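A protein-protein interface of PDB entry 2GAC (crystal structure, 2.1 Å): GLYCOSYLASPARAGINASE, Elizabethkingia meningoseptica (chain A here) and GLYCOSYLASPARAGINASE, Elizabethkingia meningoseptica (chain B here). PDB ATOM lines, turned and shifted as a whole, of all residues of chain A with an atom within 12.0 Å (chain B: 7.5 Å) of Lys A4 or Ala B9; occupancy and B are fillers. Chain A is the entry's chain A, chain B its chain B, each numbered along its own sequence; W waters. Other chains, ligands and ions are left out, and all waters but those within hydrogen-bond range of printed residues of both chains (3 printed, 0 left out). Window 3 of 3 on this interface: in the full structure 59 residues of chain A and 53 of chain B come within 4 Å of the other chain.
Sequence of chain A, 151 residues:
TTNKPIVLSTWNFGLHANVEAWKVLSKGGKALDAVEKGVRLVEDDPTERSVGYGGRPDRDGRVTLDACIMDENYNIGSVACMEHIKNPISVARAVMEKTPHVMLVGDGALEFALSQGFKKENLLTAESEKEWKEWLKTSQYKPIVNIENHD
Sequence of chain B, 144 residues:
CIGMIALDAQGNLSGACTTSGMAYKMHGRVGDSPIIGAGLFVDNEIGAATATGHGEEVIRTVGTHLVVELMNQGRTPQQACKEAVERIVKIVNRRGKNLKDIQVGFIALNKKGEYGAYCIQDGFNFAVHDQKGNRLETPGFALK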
ATOM      1  N   ASN A   3      11.125 -17.013  -8.375  1.00  0.00           N
ATOM      2  CA  ASN A   3      12.533 -17.214  -8.075  1.00  0.00           C
ATOM      3  C   ASN A   3      13.295 -17.797  -9.257  1.00  0.00           C
ATOM      4  O   ASN A   3      13.545 -19.006  -9.388  1.00  0.00           O
ATOM      5  CB  ASN A   3      12.647 -18.128  -6.851  1.00  0.00           C
ATOM      6  CG  ASN A   3      14.081 -18.560  -6.598  1.00  0.00           C
ATOM      7  OD1 ASN A   3      15.024 -17.764  -6.719  1.00  0.00           O
ATOM      8  ND2 ASN A   3      14.309 -19.831  -6.339  1.00  0.00           N
ATOM      9  N   LYS A   4      13.703 -16.908 -10.154  1.00  0.00           N
ATOM     10  CA  LYS A   4      14.382 -17.296 -11.380  1.00  0.00           C
ATOM     11  C   LYS A   4      15.433 -16.243 -11.704  1.00  0.00           C
ATOM     12  O   LYS A   4      15.194 -15.080 -11.358  1.00  0.00           O
ATOM     13  CB  LYS A   4      13.392 -17.400 -12.559  1.00  0.00           C
ATOM     14  CG  LYS A   4      12.541 -16.168 -12.840  1.00  0.00           C
ATOM     15  CD  LYS A   4      11.611 -16.452 -14.002  1.00  0.00           C
ATOM     16  CE  LYS A   4      10.619 -15.322 -14.233  1.00  0.00           C
ATOM     17  NZ  LYS A   4      11.258 -14.160 -14.814  1.00  0.00           N
ATOM     18  N   PRO A   5      16.545 -16.535 -12.392  1.00  0.00           N
ATOM     19  CA  PRO A   5      16.911 -17.879 -12.811  1.00  0.00           C
ATOM     20  C   PRO A   5      17.389 -18.762 -11.656  1.00  0.00           C
ATOM     21  O   PRO A   5      17.736 -18.244 -10.589  1.00  0.00           O
ATOM     22  CB  PRO A   5      17.937 -17.611 -13.894  1.00  0.00           C
ATOM     23  CG  PRO A   5      18.620 -16.332 -13.474  1.00  0.00           C
ATOM     24  CD  PRO A   5      17.483 -15.526 -12.888  1.00  0.00           C
ATOM     25  N   ILE A   6      17.317 -20.082 -11.799  1.00  0.00           N
ATOM     26  CA  ILE A   6      17.810 -21.013 -10.793  1.00  0.00           C
ATOM     27  C   ILE A   6      18.261 -22.293 -11.502  1.00  0.00           C
ATOM     28  O   ILE A   6      17.637 -22.701 -12.491  1.00  0.00           O
ATOM     29  CB  ILE A   6      16.674 -21.266  -9.717  1.00  0.00           C
ATOM     30  CG1 ILE A   6      17.153 -22.291  -8.694  1.00  0.00           C
ATOM     31  CG2 ILE A   6      15.367 -21.687 -10.381  1.00  0.00           C
ATOM     32  CD1 ILE A   6      16.382 -22.244  -7.367  1.00  0.00           C
ATOM     33  N   VAL A   7      19.395 -22.869 -11.067  1.00  0.00           N
ATOM     34  CA  VAL A   7      19.996 -24.107 -11.574  1.00  0.00           C
ATOM     35  C   VAL A   7      20.133 -25.078 -10.410  1.00  0.00           C
ATOM     36  O   VAL A   7      20.524 -24.644  -9.314  1.00  0.00           O
ATOM     37  CB  VAL A   7      21.483 -24.105 -12.055  1.00  0.00           C
ATOM     38  CG1 VAL A   7      21.504 -24.942 -13.323  1.00  0.00           C
ATOM     39  CG2 VAL A   7      22.090 -22.718 -12.161  1.00  0.00           C
ATOM     40  N   LEU A   8      19.868 -26.368 -10.606  1.00  0.00           N
ATOM     41  CA  LEU A   8      20.181 -27.386  -9.613  1.00  0.00           C
ATOM     42  C   LEU A   8      20.895 -28.490 -10.370  1.00  0.00           C
ATOM     43  O   LEU A   8      20.521 -28.796 -11.519  1.00  0.00           O
ATOM     44  CB  LEU A   8      19.008 -28.134  -8.959  1.00  0.00           C
ATOM     45  CG  LEU A   8      17.584 -27.693  -8.670  1.00  0.00           C
ATOM     46  CD1 LEU A   8      17.082 -28.588  -7.548  1.00  0.00           C
ATOM     47  CD2 LEU A   8      17.478 -26.258  -8.198  1.00  0.00           C
ATOM     48  N   ALA A  21      26.885 -22.860 -15.523  1.00  0.00           N
ATOM     49  CA  ALA A  21      25.516 -22.650 -15.983  1.00  0.00           C
ATOM     50  C   ALA A  21      25.040 -21.234 -15.654  1.00  0.00           C
ATOM     51  O   ALA A  21      24.341 -20.581 -16.439  1.00  0.00           O
ATOM     52  CB  ALA A  21      24.571 -23.636 -15.304  1.00  0.00           C
ATOM     53  N   TRP A  22      25.482 -20.689 -14.512  1.00  0.00           N
ATOM     54  CA  TRP A  22      25.073 -19.377 -14.049  1.00  0.00           C
ATOM     55  C   TRP A  22      25.663 -18.259 -14.874  1.00  0.00           C
ATOM     56  O   TRP A  22      25.044 -17.196 -14.976  1.00  0.00           O
ATOM     57  CB  TRP A  22      25.468 -19.178 -12.595  1.00  0.00           C
ATOM     58  CG  TRP A  22      24.714 -18.034 -11.938  1.00  0.00           C
ATOM     59  CD1 TRP A  22      25.359 -16.869 -11.602  1.00  0.00           C
ATOM     60  CD2 TRP A  22      23.376 -18.013 -11.627  1.00  0.00           C
ATOM     61  NE1 TRP A  22      24.434 -16.110 -11.080  1.00  0.00           N
ATOM     62  CE2 TRP A  22      23.251 -16.739 -11.070  1.00  0.00           C
ATOM     63  CE3 TRP A  22      22.267 -18.851 -11.718  1.00  0.00           C
ATOM     64  CZ2 TRP A  22      22.025 -16.281 -10.595  1.00  0.00           C
ATOM     65  CZ3 TRP A  22      21.040 -18.401 -11.233  1.00  0.00           C
ATOM     66  CH2 TRP A  22      20.918 -17.115 -10.693  1.00  0.00           C
ATOM     67  N   LYS A  23      26.819 -18.446 -15.502  1.00  0.00           N
ATOM     68  CA  LYS A  23      27.353 -17.439 -16.393  1.00  0.00           C
ATOM     69  C   LYS A  23      26.374 -17.149 -17.535  1.00  0.00           C
ATOM     70  O   LYS A  23      26.323 -16.002 -17.998  1.00  0.00           O
ATOM     71  CB  LYS A  23      28.666 -17.906 -16.960  1.00  0.00           C
ATOM     72  CG  LYS A  23      29.776 -18.061 -15.933  1.00  0.00           C
ATOM     73  CD  LYS A  23      30.951 -18.545 -16.752  1.00  0.00           C
ATOM     74  CE  LYS A  23      32.198 -18.820 -15.939  1.00  0.00           C
ATOM     75  NZ  LYS A  23      33.098 -19.647 -16.733  1.00  0.00           N
ATOM     76  N   VAL A  24      25.609 -18.147 -17.984  1.00  0.00           N
ATOM     77  CA  VAL A  24      24.584 -17.988 -19.018  1.00  0.00           C
ATOM     78  C   VAL A  24      23.321 -17.402 -18.389  1.00  0.00           C
ATOM     79  O   VAL A  24      22.785 -16.391 -18.853  1.00  0.00           O
ATOM     80  CB  VAL A  24      24.257 -19.367 -19.678  1.00  0.00           C
ATOM     81  CG1 VAL A  24      23.111 -19.268 -20.681  1.00  0.00           C
ATOM     82  CG2 VAL A  24      25.496 -19.863 -20.406  1.00  0.00           C
ATOM     83  N   LEU A  25      22.849 -17.997 -17.293  1.00  0.00           N
ATOM     84  CA  LEU A  25      21.601 -17.594 -16.666  1.00  0.00           C
ATOM     85  C   LEU A  25      21.571 -16.193 -16.068  1.00  0.00           C
ATOM     86  O   LEU A  25      20.564 -15.485 -16.166  1.00  0.00           O
ATOM     87  CB  LEU A  25      21.238 -18.588 -15.580  1.00  0.00           C
ATOM     88  CG  LEU A  25      20.832 -20.018 -15.943  1.00  0.00           C
ATOM     89  CD1 LEU A  25      20.607 -20.775 -14.657  1.00  0.00           C
ATOM     90  CD2 LEU A  25      19.544 -20.054 -16.741  1.00  0.00           C
ATOM     91  N   SER A  26      22.669 -15.757 -15.455  1.00  0.00           N
ATOM     92  CA  SER A  26      22.713 -14.417 -14.889  1.00  0.00           C
ATOM     93  C   SER A  26      22.713 -13.365 -15.999  1.00  0.00           C
ATOM     94  O   SER A  26      22.366 -12.213 -15.764  1.00  0.00           O
ATOM     95  CB  SER A  26      23.960 -14.241 -14.018  1.00  0.00           C
ATOM     96  OG  SER A  26      25.196 -14.484 -14.681  1.00  0.00           O
ATOM     97  N   LYS A  27      23.078 -13.736 -17.228  1.00  0.00           N
ATOM     98  CA  LYS A  27      23.055 -12.800 -18.341  1.00  0.00           C
ATOM     99  C   LYS A  27      21.754 -12.889 -19.140  1.00  0.00           C
ATOM    100  O   LYS A  27      21.678 -12.421 -20.278  1.00  0.00           O
ATOM    101  CB  LYS A  27      24.240 -13.068 -19.267  1.00  0.00           C
ATOM    102  CG  LYS A  27      25.551 -12.754 -18.571  1.00  0.00           C
ATOM    103  CD  LYS A  27      26.705 -12.773 -19.552  1.00  0.00           C
ATOM    104  CE  LYS A  27      28.037 -12.960 -18.840  1.00  0.00           C
ATOM    105  NZ  LYS A  27      28.138 -14.293 -18.273  1.00  0.00           N
ATOM    106  N   GLY A  28      20.700 -13.489 -18.575  1.00  0.00           N
ATOM    107  CA  GLY A  28      19.421 -13.648 -19.250  1.00  0.00           C
ATOM    108  C   GLY A  28      19.448 -14.672 -20.386  1.00  0.00           C
ATOM    109  O   GLY A  28      18.612 -14.594 -21.310  1.00  0.00           O
ATOM    110  N   GLY A  29      20.371 -15.626 -20.366  1.00  0.00           N
ATOM    111  CA  GLY A  29      20.454 -16.661 -21.388  1.00  0.00           C
ATOM    112  C   GLY A  29      19.429 -17.785 -21.223  1.00  0.00           C
ATOM    113  O   GLY A  29      18.723 -17.905 -20.219  1.00  0.00           O
ATOM    114  N   LYS A  30      19.321 -18.594 -22.266  1.00  0.00           N
ATOM    115  CA  LYS A  30      18.414 -19.720 -22.307  1.00  0.00           C
ATOM    116  C   LYS A  30      18.869 -20.839 -21.365  1.00  0.00           C
ATOM    117  O   LYS A  30      20.057 -21.187 -21.284  1.00  0.00           O
ATOM    118  CB  LYS A  30      18.331 -20.251 -23.748  1.00  0.00           C
ATOM    119  CG  LYS A  30      17.611 -19.343 -24.753  1.00  0.00           C
ATOM    120  CD  LYS A  30      17.966 -19.651 -26.218  1.00  0.00           C
ATOM    121  CE  LYS A  30      17.463 -20.997 -26.758  1.00  0.00           C
ATOM    122  NZ  LYS A  30      17.892 -21.229 -28.128  1.00  0.00           N
ATOM    123  N   ALA A  31      17.908 -21.409 -20.653  1.00  0.00           N
ATOM    124  CA  ALA A  31      18.147 -22.551 -19.784  1.00  0.00           C
ATOM    125  C   ALA A  31      18.769 -23.671 -20.602  1.00  0.00           C
ATOM    126  O   ALA A  31      19.680 -24.335 -20.099  1.00  0.00           O
ATOM    127  CB  ALA A  31      16.847 -23.072 -19.182  1.00  0.00           C
ATOM    128  N   LEU A  32      18.382 -23.900 -21.871  1.00  0.00           N
ATOM    129  CA  LEU A  32      19.002 -24.946 -22.675  1.00  0.00           C
ATOM    130  C   LEU A  32      20.509 -24.785 -22.822  1.00  0.00           C
ATOM    131  O   LEU A  32      21.270 -25.758 -22.671  1.00  0.00           O
ATOM    132  CB  LEU A  32      18.384 -24.999 -24.092  1.00  0.00           C
ATOM    133  CG  LEU A  32      18.804 -26.175 -25.003  1.00  0.00           C
ATOM    134  CD1 LEU A  32      18.357 -27.473 -24.354  1.00  0.00           C
ATOM    135  CD2 LEU A  32      18.182 -26.055 -26.386  1.00  0.00           C
ATOM    136  N   ASP A  33      20.965 -23.547 -23.045  1.00  0.00           N
ATOM    137  CA  ASP A  33      22.384 -23.282 -23.224  1.00  0.00           C
ATOM    138  C   ASP A  33      23.132 -23.404 -21.915  1.00  0.00           C
ATOM    139  O   ASP A  33      24.238 -23.952 -21.869  1.00  0.00           O
ATOM    140  CB  ASP A  33      22.596 -21.878 -23.802  1.00  0.00           C
ATOM    141  CG  ASP A  33      22.129 -21.775 -25.244  1.00  0.00           C
ATOM    142  OD1 ASP A  33      22.449 -22.619 -26.087  1.00  0.00           O
ATOM    143  OD2 ASP A  33      21.383 -20.863 -25.565  1.00  0.00           O
ATOM    144  N   ALA A  34      22.506 -22.931 -20.837  1.00  0.00           N
ATOM    145  CA  ALA A  34      23.062 -23.028 -19.498  1.00  0.00           C
ATOM    146  C   ALA A  34      23.281 -24.456 -19.018  1.00  0.00           C
ATOM    147  O   ALA A  34      24.380 -24.763 -18.539  1.00  0.00           O
ATOM    148  CB  ALA A  34      22.141 -22.321 -18.527  1.00  0.00           C
ATOM    149  N   VAL A  35      22.309 -25.370 -19.135  1.00  0.00           N
ATOM    150  CA  VAL A  35      22.498 -26.750 -18.696  1.00  0.00           C
ATOM    151  C   VAL A  35      23.486 -27.482 -19.590  1.00  0.00           C
ATOM    152  O   VAL A  35      24.245 -28.315 -19.082  1.00  0.00           O
ATOM    153  CB  VAL A  35      21.154 -27.547 -18.653  1.00  0.00           C
ATOM    154  CG1 VAL A  35      20.261 -26.807 -17.675  1.00  0.00           C
ATOM    155  CG2 VAL A  35      20.452 -27.685 -19.999  1.00  0.00           C
ATOM    156  N   GLU A  72      12.437 -26.579 -23.262  1.00  0.00           N
ATOM    157  CA  GLU A  72      11.174 -26.103 -22.707  1.00  0.00           C
ATOM    158  C   GLU A  72       9.931 -26.414 -23.520  1.00  0.00           C
ATOM    159  O   GLU A  72       8.821 -26.104 -23.083  1.00  0.00           O
ATOM    160  CB  GLU A  72      11.200 -24.590 -22.501  1.00  0.00           C
ATOM    161  CG  GLU A  72      11.158 -23.708 -23.754  1.00  0.00           C
ATOM    162  CD  GLU A  72      12.384 -23.667 -24.646  1.00  0.00           C
ATOM    163  OE1 GLU A  72      13.469 -24.114 -24.259  1.00  0.00           O
ATOM    164  OE2 GLU A  72      12.255 -23.153 -25.752  1.00  0.00           O
ATOM    165  N   LEU B   7      15.685 -23.150 -14.559  1.00  0.00           N
ATOM    166  CA  LEU B   7      14.594 -22.263 -14.936  1.00  0.00           C
ATOM    167  C   LEU B   7      15.293 -20.955 -15.312  1.00  0.00           C
ATOM    168  O   LEU B   7      16.029 -20.403 -14.481  1.00  0.00           O
ATOM    169  CB  LEU B   7      13.643 -22.021 -13.760  1.00  0.00           C
ATOM    170  CG  LEU B   7      12.470 -21.051 -13.921  1.00  0.00           C
ATOM    171  CD1 LEU B   7      11.467 -21.608 -14.901  1.00  0.00           C
ATOM    172  CD2 LEU B   7      11.753 -20.890 -12.597  1.00  0.00           C
ATOM    173  N   ASP B   8      15.148 -20.422 -16.521  1.00  0.00           N
ATOM    174  CA  ASP B   8      15.840 -19.197 -16.884  1.00  0.00           C
ATOM    175  C   ASP B   8      15.052 -17.931 -16.566  1.00  0.00           C
ATOM    176  O   ASP B   8      13.947 -17.974 -16.013  1.00  0.00           O
ATOM    177  CB  ASP B   8      16.203 -19.247 -18.394  1.00  0.00           C
ATOM    178  CG  ASP B   8      15.089 -19.356 -19.426  1.00  0.00           C
ATOM    179  OD1 ASP B   8      13.987 -18.889 -19.194  1.00  0.00           O
ATOM    180  OD2 ASP B   8      15.351 -19.866 -20.502  1.00  0.00           O
ATOM    181  N   ALA B   9      15.561 -16.741 -16.882  1.00  0.00           N
ATOM    182  CA  ALA B   9      14.834 -15.507 -16.616  1.00  0.00           C
ATOM    183  C   ALA B   9      13.543 -15.332 -17.424  1.00  0.00           C
ATOM    184  O   ALA B   9      12.621 -14.617 -16.998  1.00  0.00           O
ATOM    185  CB  ALA B   9      15.785 -14.355 -16.878  1.00  0.00           C
ATOM    186  N   GLN B  10      13.368 -16.019 -18.548  1.00  0.00           N
ATOM    187  CA  GLN B  10      12.132 -15.967 -19.303  1.00  0.00           C
ATOM    188  C   GLN B  10      11.151 -16.893 -18.603  1.00  0.00           C
ATOM    189  O   GLN B  10       9.962 -16.859 -18.911  1.00  0.00           O
ATOM    190  CB  GLN B  10      12.316 -16.470 -20.732  1.00  0.00           C
ATOM    191  CG  GLN B  10      13.330 -15.703 -21.564  1.00  0.00           C
ATOM    192  CD  GLN B  10      13.825 -16.448 -22.796  1.00  0.00           C
ATOM    193  OE1 GLN B  10      13.204 -16.484 -23.871  1.00  0.00           O
ATOM    194  NE2 GLN B  10      15.022 -17.006 -22.719  1.00  0.00           N
ATOM    195  N   GLY B  11      11.575 -17.726 -17.646  1.00  0.00           N
ATOM    196  CA  GLY B  11      10.659 -18.647 -17.010  1.00  0.00           C
ATOM    197  C   GLY B  11      10.572 -19.955 -17.804  1.00  0.00           C
ATOM    198  O   GLY B  11       9.556 -20.652 -17.709  1.00  0.00           O
ATOM    199  N   ASN B  12      11.589 -20.373 -18.550  1.00  0.00           N
ATOM    200  CA  ASN B  12      11.549 -21.626 -19.286  1.00  0.00           C
ATOM    201  C   ASN B  12      12.515 -22.592 -18.649  1.00  0.00           C
ATOM    202  O   ASN B  12      13.544 -22.207 -18.091  1.00  0.00           O
ATOM    203  CB  ASN B  12      11.958 -21.474 -20.753  1.00  0.00           C
ATOM    204  CG  ASN B  12      10.967 -20.681 -21.599  1.00  0.00           C
ATOM    205  OD1 ASN B  12       9.761 -20.703 -21.376  1.00  0.00           O
ATOM    206  ND2 ASN B  12      11.436 -19.960 -22.603  1.00  0.00           N
ATOM    207  N   LYS B 111       7.745 -24.485 -12.054  1.00  0.00           N
ATOM    208  CA  LYS B 111       7.684 -23.178 -12.685  1.00  0.00           C
ATOM    209  C   LYS B 111       7.850 -21.942 -11.797  1.00  0.00           C
ATOM    210  O   LYS B 111       8.279 -20.896 -12.275  1.00  0.00           O
ATOM    211  CB  LYS B 111       6.373 -23.099 -13.448  1.00  0.00           C
ATOM    212  CG  LYS B 111       6.427 -24.039 -14.651  1.00  0.00           C
ATOM    213  CD  LYS B 111       7.572 -23.680 -15.605  1.00  0.00           C
ATOM    214  CE  LYS B 111       7.480 -22.331 -16.315  1.00  0.00           C
ATOM    215  NZ  LYS B 111       6.276 -22.163 -17.115  1.00  0.00           N
ATOM    216  N   LYS B 112       7.525 -22.008 -10.503  1.00  0.00           N
ATOM    217  CA  LYS B 112       7.744 -20.883  -9.622  1.00  0.00           C
ATOM    218  C   LYS B 112       9.208 -20.820  -9.206  1.00  0.00           C
ATOM    219  O   LYS B 112       9.605 -19.852  -8.559  1.00  0.00           O
ATOM    220  CB  LYS B 112       6.947 -20.963  -8.322  1.00  0.00           C
ATOM    221  CG  LYS B 112       5.437 -20.973  -8.442  1.00  0.00           C
ATOM    222  CD  LYS B 112       4.846 -20.659  -7.071  1.00  0.00           C
ATOM    223  CE  LYS B 112       3.778 -21.658  -6.620  1.00  0.00           C
ATOM    224  NZ  LYS B 112       4.302 -22.855  -5.970  1.00  0.00           N
ATOM    225  N   GLY B 113      10.031 -21.823  -9.503  1.00  0.00           N
ATOM    226  CA  GLY B 113      11.404 -21.786  -9.034  1.00  0.00           C
ATOM    227  C   GLY B 113      11.526 -22.385  -7.645  1.00  0.00           C
ATOM    228  O   GLY B 113      12.549 -22.208  -6.967  1.00  0.00           O
ATOM    229  N   ASP B 130      20.745 -19.869  -7.239  1.00  0.00           N
ATOM    230  CA  ASP B 130      19.775 -18.854  -7.624  1.00  0.00           C
ATOM    231  C   ASP B 130      20.422 -17.499  -7.299  1.00  0.00           C
ATOM    232  O   ASP B 130      21.663 -17.429  -7.186  1.00  0.00           O
ATOM    233  CB  ASP B 130      18.451 -19.054  -6.849  1.00  0.00           C
ATOM    234  CG  ASP B 130      18.500 -19.031  -5.330  1.00  0.00           C
ATOM    235  OD1 ASP B 130      19.503 -18.658  -4.734  1.00  0.00           O
ATOM    236  OD2 ASP B 130      17.548 -19.441  -4.683  1.00  0.00           O
ATOM    237  N   GLN B 131      19.644 -16.460  -6.954  1.00  0.00           N
ATOM    238  CA  GLN B 131      20.148 -15.165  -6.493  1.00  0.00           C
ATOM    239  C   GLN B 131      20.654 -15.155  -5.040  1.00  0.00           C
ATOM    240  O   GLN B 131      21.044 -14.112  -4.516  1.00  0.00           O
ATOM    241  CB  GLN B 131      19.083 -14.072  -6.567  1.00  0.00           C
ATOM    242  CG  GLN B 131      18.248 -13.936  -7.827  1.00  0.00           C
ATOM    243  CD  GLN B 131      18.960 -13.648  -9.138  1.00  0.00           C
ATOM    244  OE1 GLN B 131      20.187 -13.645  -9.281  1.00  0.00           O
ATOM    245  NE2 GLN B 131      18.166 -13.431 -10.171  1.00  0.00           N
HETATM  246  O   HOH W   1      16.331 -16.211 -20.352  1.00  0.00           O
HETATM  247  O   HOH W   2      18.409 -16.622 -17.920  1.00  0.00           O
HETATM  248  O   HOH W   3      16.851 -16.454  -8.493  1.00  0.00           O
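The backbone carbonyl oxygen (O) of Trp A22 sits at hydrogen-bond distance from the side-chain hydroxyl (OG) of Ser A26 (2.7 Å). The backbone NH (N) of Gly A29 sits at hydrogen-bond distance from the backbone carbonyl oxygen (O) of Val A24 (2.9 Å). The side-chain carboxylate (OD1) of Asp B8 is in hydrogen-bond range of the backbone NH (N) of Gln B10 (3.0 Å). The backbone NH of Gly B11 sits at hydrogen-bond distance from the side-chain carboxylate of Asp B8 (3.1 Å). N of Asn B12 lies within hydrogen-bond range of OD1 of Asp B8 (2.9 Å).
Of the printed residues of chain B, Asn A3 touches Lys B112 (3.2 Å), Gly B113 (3.0 Å) and Asp B130 (3.7 Å). Of chain B, only Leu B7, Asp B8, Ala B9, Gly B11 and Gln B131 come within 4 Å of Lys A4. Printed residues of chain B within 4 Å of Pro A5: Leu B7 (3.2 Å), Asp B8 (3.9 Å), Ala B9 (3.9 Å), Asp B130 (3.6 Å) and Gln B131 (3.5 Å). Printed residues of chain B within 4 Å of Ile A6: Leu B7, Gly B113 and Asp B130. Of the printed residues of chain B, Trp A22 touches Asp B130 (3.5 Å) and Gln B131 (3.5 Å). Of the printed residues of chain B, Gly A29 touches Asp B8 (3.4 Å). Leu A32 touches none of the printed residues of chain B. Asp A33 touches none of the printed residues of chain B. Of chain A, only Lys A4 (3.4 Å), Pro A5 (3.9 Å), Leu A25 (3.8 Å), Gly A29 (3.4 Å), Lys A30 (3.6 Å) and Ala A31 (3.0 Å) come within 4 Å of Asp B8. Ala B9 touches just these residues of chain A: Lys A4 and Pro A5. No residue of chain A comes within 4 Å of Gln B10. Of the printed residues of chain A, Gly B11 touches Lys A4. The nearest residue of chain B that does not touch Lys A4 is Gln B10 (4.6 Å).
Water W2 lies within hydrogen-bond range of O of Gly A29, O of Leu A25 and N of Ala B9. Water W1 lies within hydrogen-bond range of NE2 of Gln B10 (2.8 Å), O of Gly A29 (2.9 Å) and O of Gly A28 (3.0 Å). Water W3 lies within hydrogen-bond range of OD1 of Asn A3 (2.9 Å), O of Pro A5 (2.9 Å) and N of Gln B131 (3.2 Å).
Asn A3 touches Asp B130 (OD1 to OD2, 3.7 Å). CB of Lys A4 touches CD2 of Leu B7, at 3.9 Å. Lys A4 touches Gln B131. O of Leu B7 touches CA of Pro A5 (3.2 Å). C of Asp B8 touches CB of Pro A5, at 3.9 Å. O of Gly B113 touches CD1 of Ile A6 (3.9 Å). C of Asp B130 touches CH2 of Trp A22, at 3.5 Å. Gly A29 touches Asp B8 (O to CB, 3.4 Å). CA of Lys A30 touches OD2 of Asp B8, at 3.6 Å. CB of Glu A72 touches CB of Asn B12, at 3.7 Å.
O of Lys B112 sits at hydrogen-bond distance from N of Asn A3, at 3.2 Å. ND2 of Asn A3 is in hydrogen-bond range of O of Gly B113, 3.0 Å away. The side-chain amino group (NZ) of Lys A4 is in hydrogen-bond range of the backbone carbonyl oxygen (O) of Ala B9 (2.6 Å). The backbone carbonyl oxygen (O) of Ile A6 sits at hydrogen-bond distance from the backbone NH (N) of Leu B7 (2.9 Å). The backbone NH of Ala A31 lies within hydrogen-bond range of the side-chain carboxylate of Asp B8 (3.0 Å).
Hydrophobic or aromatic side chains of chain B within 4 Å of the printed part of chain A: Leu B7. Hydrophobic or aromatic side chains of chain A within 4 Å of the printed part of chain B: Pro A5, Ile A6, Trp A22, Leu A25 and Ala A31. Among the printed residues, 24 pairs touch across the chains. Among the printed residues, no Asp or Glu carboxylate lies within 4 Å of a Lys or Arg side-chain nitrogen of the other chain.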
